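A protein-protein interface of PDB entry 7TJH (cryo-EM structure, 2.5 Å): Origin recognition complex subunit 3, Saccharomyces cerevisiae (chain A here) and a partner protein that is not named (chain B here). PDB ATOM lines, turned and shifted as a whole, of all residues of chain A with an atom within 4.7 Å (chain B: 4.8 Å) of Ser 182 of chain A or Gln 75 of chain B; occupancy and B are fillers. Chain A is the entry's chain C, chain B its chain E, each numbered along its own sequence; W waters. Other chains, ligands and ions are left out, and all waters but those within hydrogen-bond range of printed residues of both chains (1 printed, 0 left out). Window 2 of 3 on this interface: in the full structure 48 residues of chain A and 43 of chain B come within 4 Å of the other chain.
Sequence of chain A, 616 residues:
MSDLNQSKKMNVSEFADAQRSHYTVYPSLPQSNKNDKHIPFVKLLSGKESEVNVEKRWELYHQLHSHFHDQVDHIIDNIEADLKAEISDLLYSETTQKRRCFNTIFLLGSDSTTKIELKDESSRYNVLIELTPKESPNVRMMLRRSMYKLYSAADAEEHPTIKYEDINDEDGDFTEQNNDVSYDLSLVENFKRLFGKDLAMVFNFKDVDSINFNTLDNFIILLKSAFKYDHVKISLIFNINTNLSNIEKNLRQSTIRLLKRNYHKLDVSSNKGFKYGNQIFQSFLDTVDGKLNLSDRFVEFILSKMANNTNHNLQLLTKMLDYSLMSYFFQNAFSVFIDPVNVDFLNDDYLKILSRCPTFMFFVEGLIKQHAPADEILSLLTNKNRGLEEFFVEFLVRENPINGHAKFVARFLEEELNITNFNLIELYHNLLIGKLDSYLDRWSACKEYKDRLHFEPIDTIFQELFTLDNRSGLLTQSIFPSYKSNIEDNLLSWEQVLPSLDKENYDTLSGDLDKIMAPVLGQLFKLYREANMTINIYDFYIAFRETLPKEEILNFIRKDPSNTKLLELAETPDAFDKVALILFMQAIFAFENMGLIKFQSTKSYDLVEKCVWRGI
The side-chain amide oxygen of Gln 75 of chain B is in hydrogen-bond range of the side-chain hydroxyl of Ser 182 of chain A (3.5 Å).
The side-chain hydroxyl (OG) of Ser 182 of chain A sits at hydrogen-bond distance from the side-chain carboxylate (OD2) of Asp 184 of chain A (2.4 Å). NE2 of Gln 75 of chain B lies within hydrogen-bond range of O of Val 102 of chain B, 3.3 Å away. The side-chain amino group of Lys 71 of chain B sits close to the side-chain amide nitrogen of Gln 75 of chain B (3.4 Å).
Asp 180 of chain A touches Leu 100 of chain B. Val 181 of chain A touches Leu 100 of chain B. Pro 72 of chain B touches Ser 182 of chain A. Pro 72 of chain B touches Asp 184 of chain A (CB to OD2, 3.7 Å).
Of the printed residues of chain B, Asp 180 of chain A touches Leu 100. Of the printed residues of chain B, Val 181 of chain A touches Leu 100 (3.9 Å). Of the printed residues of chain A, Pro 72 of chain B touches Ser 182 (3.9 Å) and Asp 184 (3.7 Å). Gln 75 of chain B touches just one residue of chain A: Ser 182 (3.5 Å). The nearest printed residue of chain A that does not touch Gln 75 of chain B is Asp 184 of chain A (5.5 Å). The nearest printed residue of chain A that does not touch Leu 100 of chain B is Ser 182 of chain A (4.4 Å).
Of the 12 printed residues of chain B, 3 touch a printed residue of chain A. Hydrophobic or aromatic side chains of chain B that line the printed part of chain A: Pro 72 and Leu 100. Along chain B the printed residues that touch a printed residue of chain A span positions 72 to 100. Of the 6 printed residues of chain A, 4 touch a printed residue of chain B. Among the printed residues, 5 pairs touch across the chains.
Water W1 lies within hydrogen-bond range of NH2 of Arg 79 of chain B (2.6 Å), O of Pro 72 of chain B (3.0 Å) and OD2 of Asp 184 of chain A (3.2 Å).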
ATOM      1  N   ASP A 180      14.070 -17.644 -26.874  1.00  0.00           N
ATOM      2  CA  ASP A 180      13.052 -17.723 -25.841  1.00  0.00           C
ATOM      3  C   ASP A 180      12.688 -19.180 -25.584  1.00  0.00           C
ATOM      4  O   ASP A 180      12.961 -20.065 -26.399  1.00  0.00           O
ATOM      5  CB  ASP A 180      11.803 -16.925 -26.231  1.00  0.00           C
ATOM      6  CG  ASP A 180      12.101 -15.460 -26.496  1.00  0.00           C
ATOM      7  OD1 ASP A 180      12.083 -14.667 -25.530  1.00  0.00           O
ATOM      8  OD2 ASP A 180      12.346 -15.100 -27.667  1.00  0.00           O
ATOM      9  N   VAL A 181      12.070 -19.422 -24.429  1.00  0.00           N
ATOM     10  CA  VAL A 181      11.724 -20.768 -23.990  1.00  0.00           C
ATOM     11  C   VAL A 181      10.281 -20.779 -23.508  1.00  0.00           C
ATOM     12  O   VAL A 181       9.675 -19.739 -23.247  1.00  0.00           O
ATOM     13  CB  VAL A 181      12.649 -21.284 -22.863  1.00  0.00           C
ATOM     14  CG1 VAL A 181      14.037 -21.598 -23.392  1.00  0.00           C
ATOM     15  CG2 VAL A 181      12.713 -20.278 -21.723  1.00  0.00           C
ATOM     16  N   SER A 182       9.740 -21.984 -23.386  1.00  0.00           N
ATOM     17  CA  SER A 182       8.434 -22.193 -22.783  1.00  0.00           C
ATOM     18  C   SER A 182       8.608 -22.394 -21.282  1.00  0.00           C
ATOM     19  O   SER A 182       9.448 -23.192 -20.852  1.00  0.00           O
ATOM     20  CB  SER A 182       7.741 -23.397 -23.417  1.00  0.00           C
ATOM     21  OG  SER A 182       6.571 -23.752 -22.705  1.00  0.00           O
ATOM     22  N   TYR A 183       7.817 -21.668 -20.487  1.00  0.00           N
ATOM     23  CA  TYR A 183       7.989 -21.639 -19.033  1.00  0.00           C
ATOM     24  C   TYR A 183       7.251 -22.813 -18.385  1.00  0.00           C
ATOM     25  O   TYR A 183       6.280 -22.660 -17.641  1.00  0.00           O
ATOM     26  CB  TYR A 183       7.528 -20.303 -18.468  1.00  0.00           C
ATOM     27  CG  TYR A 183       8.442 -19.164 -18.842  1.00  0.00           C
ATOM     28  CD1 TYR A 183       9.824 -19.309 -18.770  1.00  0.00           C
ATOM     29  CD2 TYR A 183       7.929 -17.953 -19.292  1.00  0.00           C
ATOM     30  CE1 TYR A 183      10.670 -18.278 -19.123  1.00  0.00           C
ATOM     31  CE2 TYR A 183       8.766 -16.915 -19.651  1.00  0.00           C
ATOM     32  CZ  TYR A 183      10.136 -17.085 -19.563  1.00  0.00           C
ATOM     33  OH  TYR A 183      10.973 -16.055 -19.917  1.00  0.00           O
ATOM     34  N   ASP A 184       7.746 -24.011 -18.679  1.00  0.00           N
ATOM     35  CA  ASP A 184       7.259 -25.228 -18.048  1.00  0.00           C
ATOM     36  C   ASP A 184       8.443 -26.104 -17.656  1.00  0.00           C
ATOM     37  O   ASP A 184       9.598 -25.690 -17.799  1.00  0.00           O
ATOM     38  CB  ASP A 184       6.292 -25.968 -18.977  1.00  0.00           C
ATOM     39  CG  ASP A 184       6.948 -26.422 -20.263  1.00  0.00           C
ATOM     40  OD1 ASP A 184       7.586 -27.493 -20.263  1.00  0.00           O
ATOM     41  OD2 ASP A 184       6.814 -25.717 -21.281  1.00  0.00           O
ATOM     42  N   LEU A 187      12.059 -27.014 -19.548  1.00  0.00           N
ATOM     43  CA  LEU A 187      13.260 -26.208 -19.351  1.00  0.00           C
ATOM     44  C   LEU A 187      14.168 -26.826 -18.293  1.00  0.00           C
ATOM     45  O   LEU A 187      15.398 -26.770 -18.411  1.00  0.00           O
ATOM     46  CB  LEU A 187      12.864 -24.780 -18.970  1.00  0.00           C
ATOM     47  CG  LEU A 187      13.885 -23.858 -18.298  1.00  0.00           C
ATOM     48  CD1 LEU A 187      14.999 -23.481 -19.262  1.00  0.00           C
ATOM     49  CD2 LEU A 187      13.206 -22.623 -17.745  1.00  0.00           C
ATOM     50  N   LYS B  71      -1.287 -25.138 -24.597  1.00  0.00           N
ATOM     51  CA  LYS B  71      -0.291 -24.466 -25.434  1.00  0.00           C
ATOM     52  C   LYS B  71       1.144 -24.962 -25.219  1.00  0.00           C
ATOM     53  O   LYS B  71       1.836 -25.197 -26.231  1.00  0.00           O
ATOM     54  CB  LYS B  71      -0.428 -22.946 -25.256  1.00  0.00           C
ATOM     55  CG  LYS B  71       0.490 -22.112 -26.125  1.00  0.00           C
ATOM     56  CD  LYS B  71      -0.187 -20.824 -26.550  1.00  0.00           C
ATOM     57  CE  LYS B  71       0.410 -19.626 -25.838  1.00  0.00           C
ATOM     58  NZ  LYS B  71       1.779 -19.317 -26.332  1.00  0.00           N
ATOM     59  N   PRO B  72       1.660 -25.152 -23.983  1.00  0.00           N
ATOM     60  CA  PRO B  72       2.964 -25.827 -23.862  1.00  0.00           C
ATOM     61  C   PRO B  72       2.971 -27.253 -24.379  1.00  0.00           C
ATOM     62  O   PRO B  72       4.018 -27.716 -24.833  1.00  0.00           O
ATOM     63  CB  PRO B  72       3.250 -25.780 -22.354  1.00  0.00           C
ATOM     64  CG  PRO B  72       2.483 -24.657 -21.868  1.00  0.00           C
ATOM     65  CD  PRO B  72       1.227 -24.687 -22.644  1.00  0.00           C
ATOM     66  N   LEU B  73       1.834 -27.953 -24.345  1.00  0.00           N
ATOM     67  CA  LEU B  73       1.778 -29.299 -24.911  1.00  0.00           C
ATOM     68  C   LEU B  73       1.924 -29.270 -26.432  1.00  0.00           C
ATOM     69  O   LEU B  73       2.645 -30.099 -26.999  1.00  0.00           O
ATOM     70  CB  LEU B  73       0.479 -29.986 -24.491  1.00  0.00           C
ATOM     71  CG  LEU B  73       0.163 -31.376 -25.052  1.00  0.00           C
ATOM     72  CD1 LEU B  73       1.280 -32.374 -24.780  1.00  0.00           C
ATOM     73  CD2 LEU B  73      -1.158 -31.881 -24.490  1.00  0.00           C
ATOM     74  N   LEU B  74       1.268 -28.311 -27.100  1.00  0.00           N
ATOM     75  CA  LEU B  74       1.429 -28.150 -28.548  1.00  0.00           C
ATOM     76  C   LEU B  74       2.865 -27.789 -28.914  1.00  0.00           C
ATOM     77  O   LEU B  74       3.439 -28.344 -29.870  1.00  0.00           O
ATOM     78  CB  LEU B  74       0.474 -27.074 -29.068  1.00  0.00           C
ATOM     79  CG  LEU B  74      -1.039 -27.200 -28.877  1.00  0.00           C
ATOM     80  CD1 LEU B  74      -1.738 -25.916 -29.280  1.00  0.00           C
ATOM     81  CD2 LEU B  74      -1.599 -28.368 -29.654  1.00  0.00           C
ATOM     82  N   GLN B  75       3.469 -26.878 -28.143  1.00  0.00           N
ATOM     83  CA  GLN B  75       4.856 -26.491 -28.383  1.00  0.00           C
ATOM     84  C   GLN B  75       5.816 -27.650 -28.127  1.00  0.00           C
ATOM     85  O   GLN B  75       6.801 -27.818 -28.857  1.00  0.00           O
ATOM     86  CB  GLN B  75       5.212 -25.281 -27.523  1.00  0.00           C
ATOM     87  CG  GLN B  75       4.412 -24.050 -27.888  1.00  0.00           C
ATOM     88  CD  GLN B  75       4.539 -22.934 -26.881  1.00  0.00           C
ATOM     89  OE1 GLN B  75       5.150 -23.095 -25.828  1.00  0.00           O
ATOM     90  NE2 GLN B  75       3.947 -21.792 -27.195  1.00  0.00           N
ATOM     91  N   ALA B  76       5.522 -28.478 -27.121  1.00  0.00           N
ATOM     92  CA  ALA B  76       6.346 -29.646 -26.835  1.00  0.00           C
ATOM     93  C   ALA B  76       6.232 -30.690 -27.936  1.00  0.00           C
ATOM     94  O   ALA B  76       7.224 -31.348 -28.267  1.00  0.00           O
ATOM     95  CB  ALA B  76       5.952 -30.246 -25.485  1.00  0.00           C
ATOM     96  N   ILE B  77       5.035 -30.846 -28.513  1.00  0.00           N
ATOM     97  CA  ILE B  77       4.851 -31.763 -29.636  1.00  0.00           C
ATOM     98  C   ILE B  77       5.694 -31.327 -30.826  1.00  0.00           C
ATOM     99  O   ILE B  77       6.432 -32.133 -31.407  1.00  0.00           O
ATOM    100  CB  ILE B  77       3.360 -31.869 -30.007  1.00  0.00           C
ATOM    101  CG1 ILE B  77       2.624 -32.712 -28.976  1.00  0.00           C
ATOM    102  CG2 ILE B  77       3.169 -32.447 -31.408  1.00  0.00           C
ATOM    103  CD1 ILE B  77       1.183 -32.427 -28.914  1.00  0.00           C
ATOM    104  N   ALA B  78       5.643 -30.029 -31.161  1.00  0.00           N
ATOM    105  CA  ALA B  78       6.421 -29.527 -32.296  1.00  0.00           C
ATOM    106  C   ALA B  78       7.926 -29.641 -32.050  1.00  0.00           C
ATOM    107  O   ALA B  78       8.665 -30.133 -32.919  1.00  0.00           O
ATOM    108  CB  ALA B  78       6.036 -28.082 -32.598  1.00  0.00           C
ATOM    109  N   ARG B  79       8.374 -29.290 -30.837  1.00  0.00           N
ATOM    110  CA  ARG B  79       9.794 -29.322 -30.498  1.00  0.00           C
ATOM    111  C   ARG B  79      10.344 -30.744 -30.503  1.00  0.00           C
ATOM    112  O   ARG B  79      11.383 -31.018 -31.120  1.00  0.00           O
ATOM    113  CB  ARG B  79      10.005 -28.670 -29.130  1.00  0.00           C
ATOM    114  CG  ARG B  79      11.451 -28.484 -28.719  1.00  0.00           C
ATOM    115  CD  ARG B  79      11.636 -28.743 -27.232  1.00  0.00           C
ATOM    116  NE  ARG B  79      10.486 -28.315 -26.442  1.00  0.00           N
ATOM    117  CZ  ARG B  79       9.965 -29.015 -25.443  1.00  0.00           C
ATOM    118  NH1 ARG B  79      10.461 -30.189 -25.088  1.00  0.00           N
ATOM    119  NH2 ARG B  79       8.915 -28.529 -24.789  1.00  0.00           N
ATOM    120  N   PRO B  99       9.374 -23.881 -32.239  1.00  0.00           N
ATOM    121  CA  PRO B  99       8.163 -24.411 -31.588  1.00  0.00           C
ATOM    122  C   PRO B  99       7.325 -23.360 -30.877  1.00  0.00           C
ATOM    123  O   PRO B  99       6.137 -23.607 -30.643  1.00  0.00           O
ATOM    124  CB  PRO B  99       8.711 -25.450 -30.596  1.00  0.00           C
ATOM    125  CG  PRO B  99      10.164 -25.188 -30.492  1.00  0.00           C
ATOM    126  CD  PRO B  99      10.598 -24.547 -31.765  1.00  0.00           C
ATOM    127  N   LEU B 100       7.882 -22.195 -30.546  1.00  0.00           N
ATOM    128  CA  LEU B 100       7.094 -21.152 -29.908  1.00  0.00           C
ATOM    129  C   LEU B 100       6.171 -20.416 -30.874  1.00  0.00           C
ATOM    130  O   LEU B 100       5.333 -19.634 -30.418  1.00  0.00           O
ATOM    131  CB  LEU B 100       8.006 -20.148 -29.210  1.00  0.00           C
ATOM    132  CG  LEU B 100       8.537 -20.582 -27.846  1.00  0.00           C
ATOM    133  CD1 LEU B 100       9.777 -19.785 -27.507  1.00  0.00           C
ATOM    134  CD2 LEU B 100       7.477 -20.421 -26.766  1.00  0.00           C
ATOM    135  N   VAL B 102       3.940 -22.019 -32.443  1.00  0.00           N
ATOM    136  CA  VAL B 102       2.707 -22.784 -32.303  1.00  0.00           C
ATOM    137  C   VAL B 102       1.922 -22.220 -31.122  1.00  0.00           C
ATOM    138  O   VAL B 102       2.278 -22.447 -29.964  1.00  0.00           O
ATOM    139  CB  VAL B 102       2.993 -24.278 -32.114  1.00  0.00           C
ATOM    140  CG1 VAL B 102       1.694 -25.057 -31.981  1.00  0.00           C
ATOM    141  CG2 VAL B 102       3.822 -24.809 -33.264  1.00  0.00           C
HETATM  142  O   HOH W   1       6.824 -27.039 -24.155  1.00  0.00           O
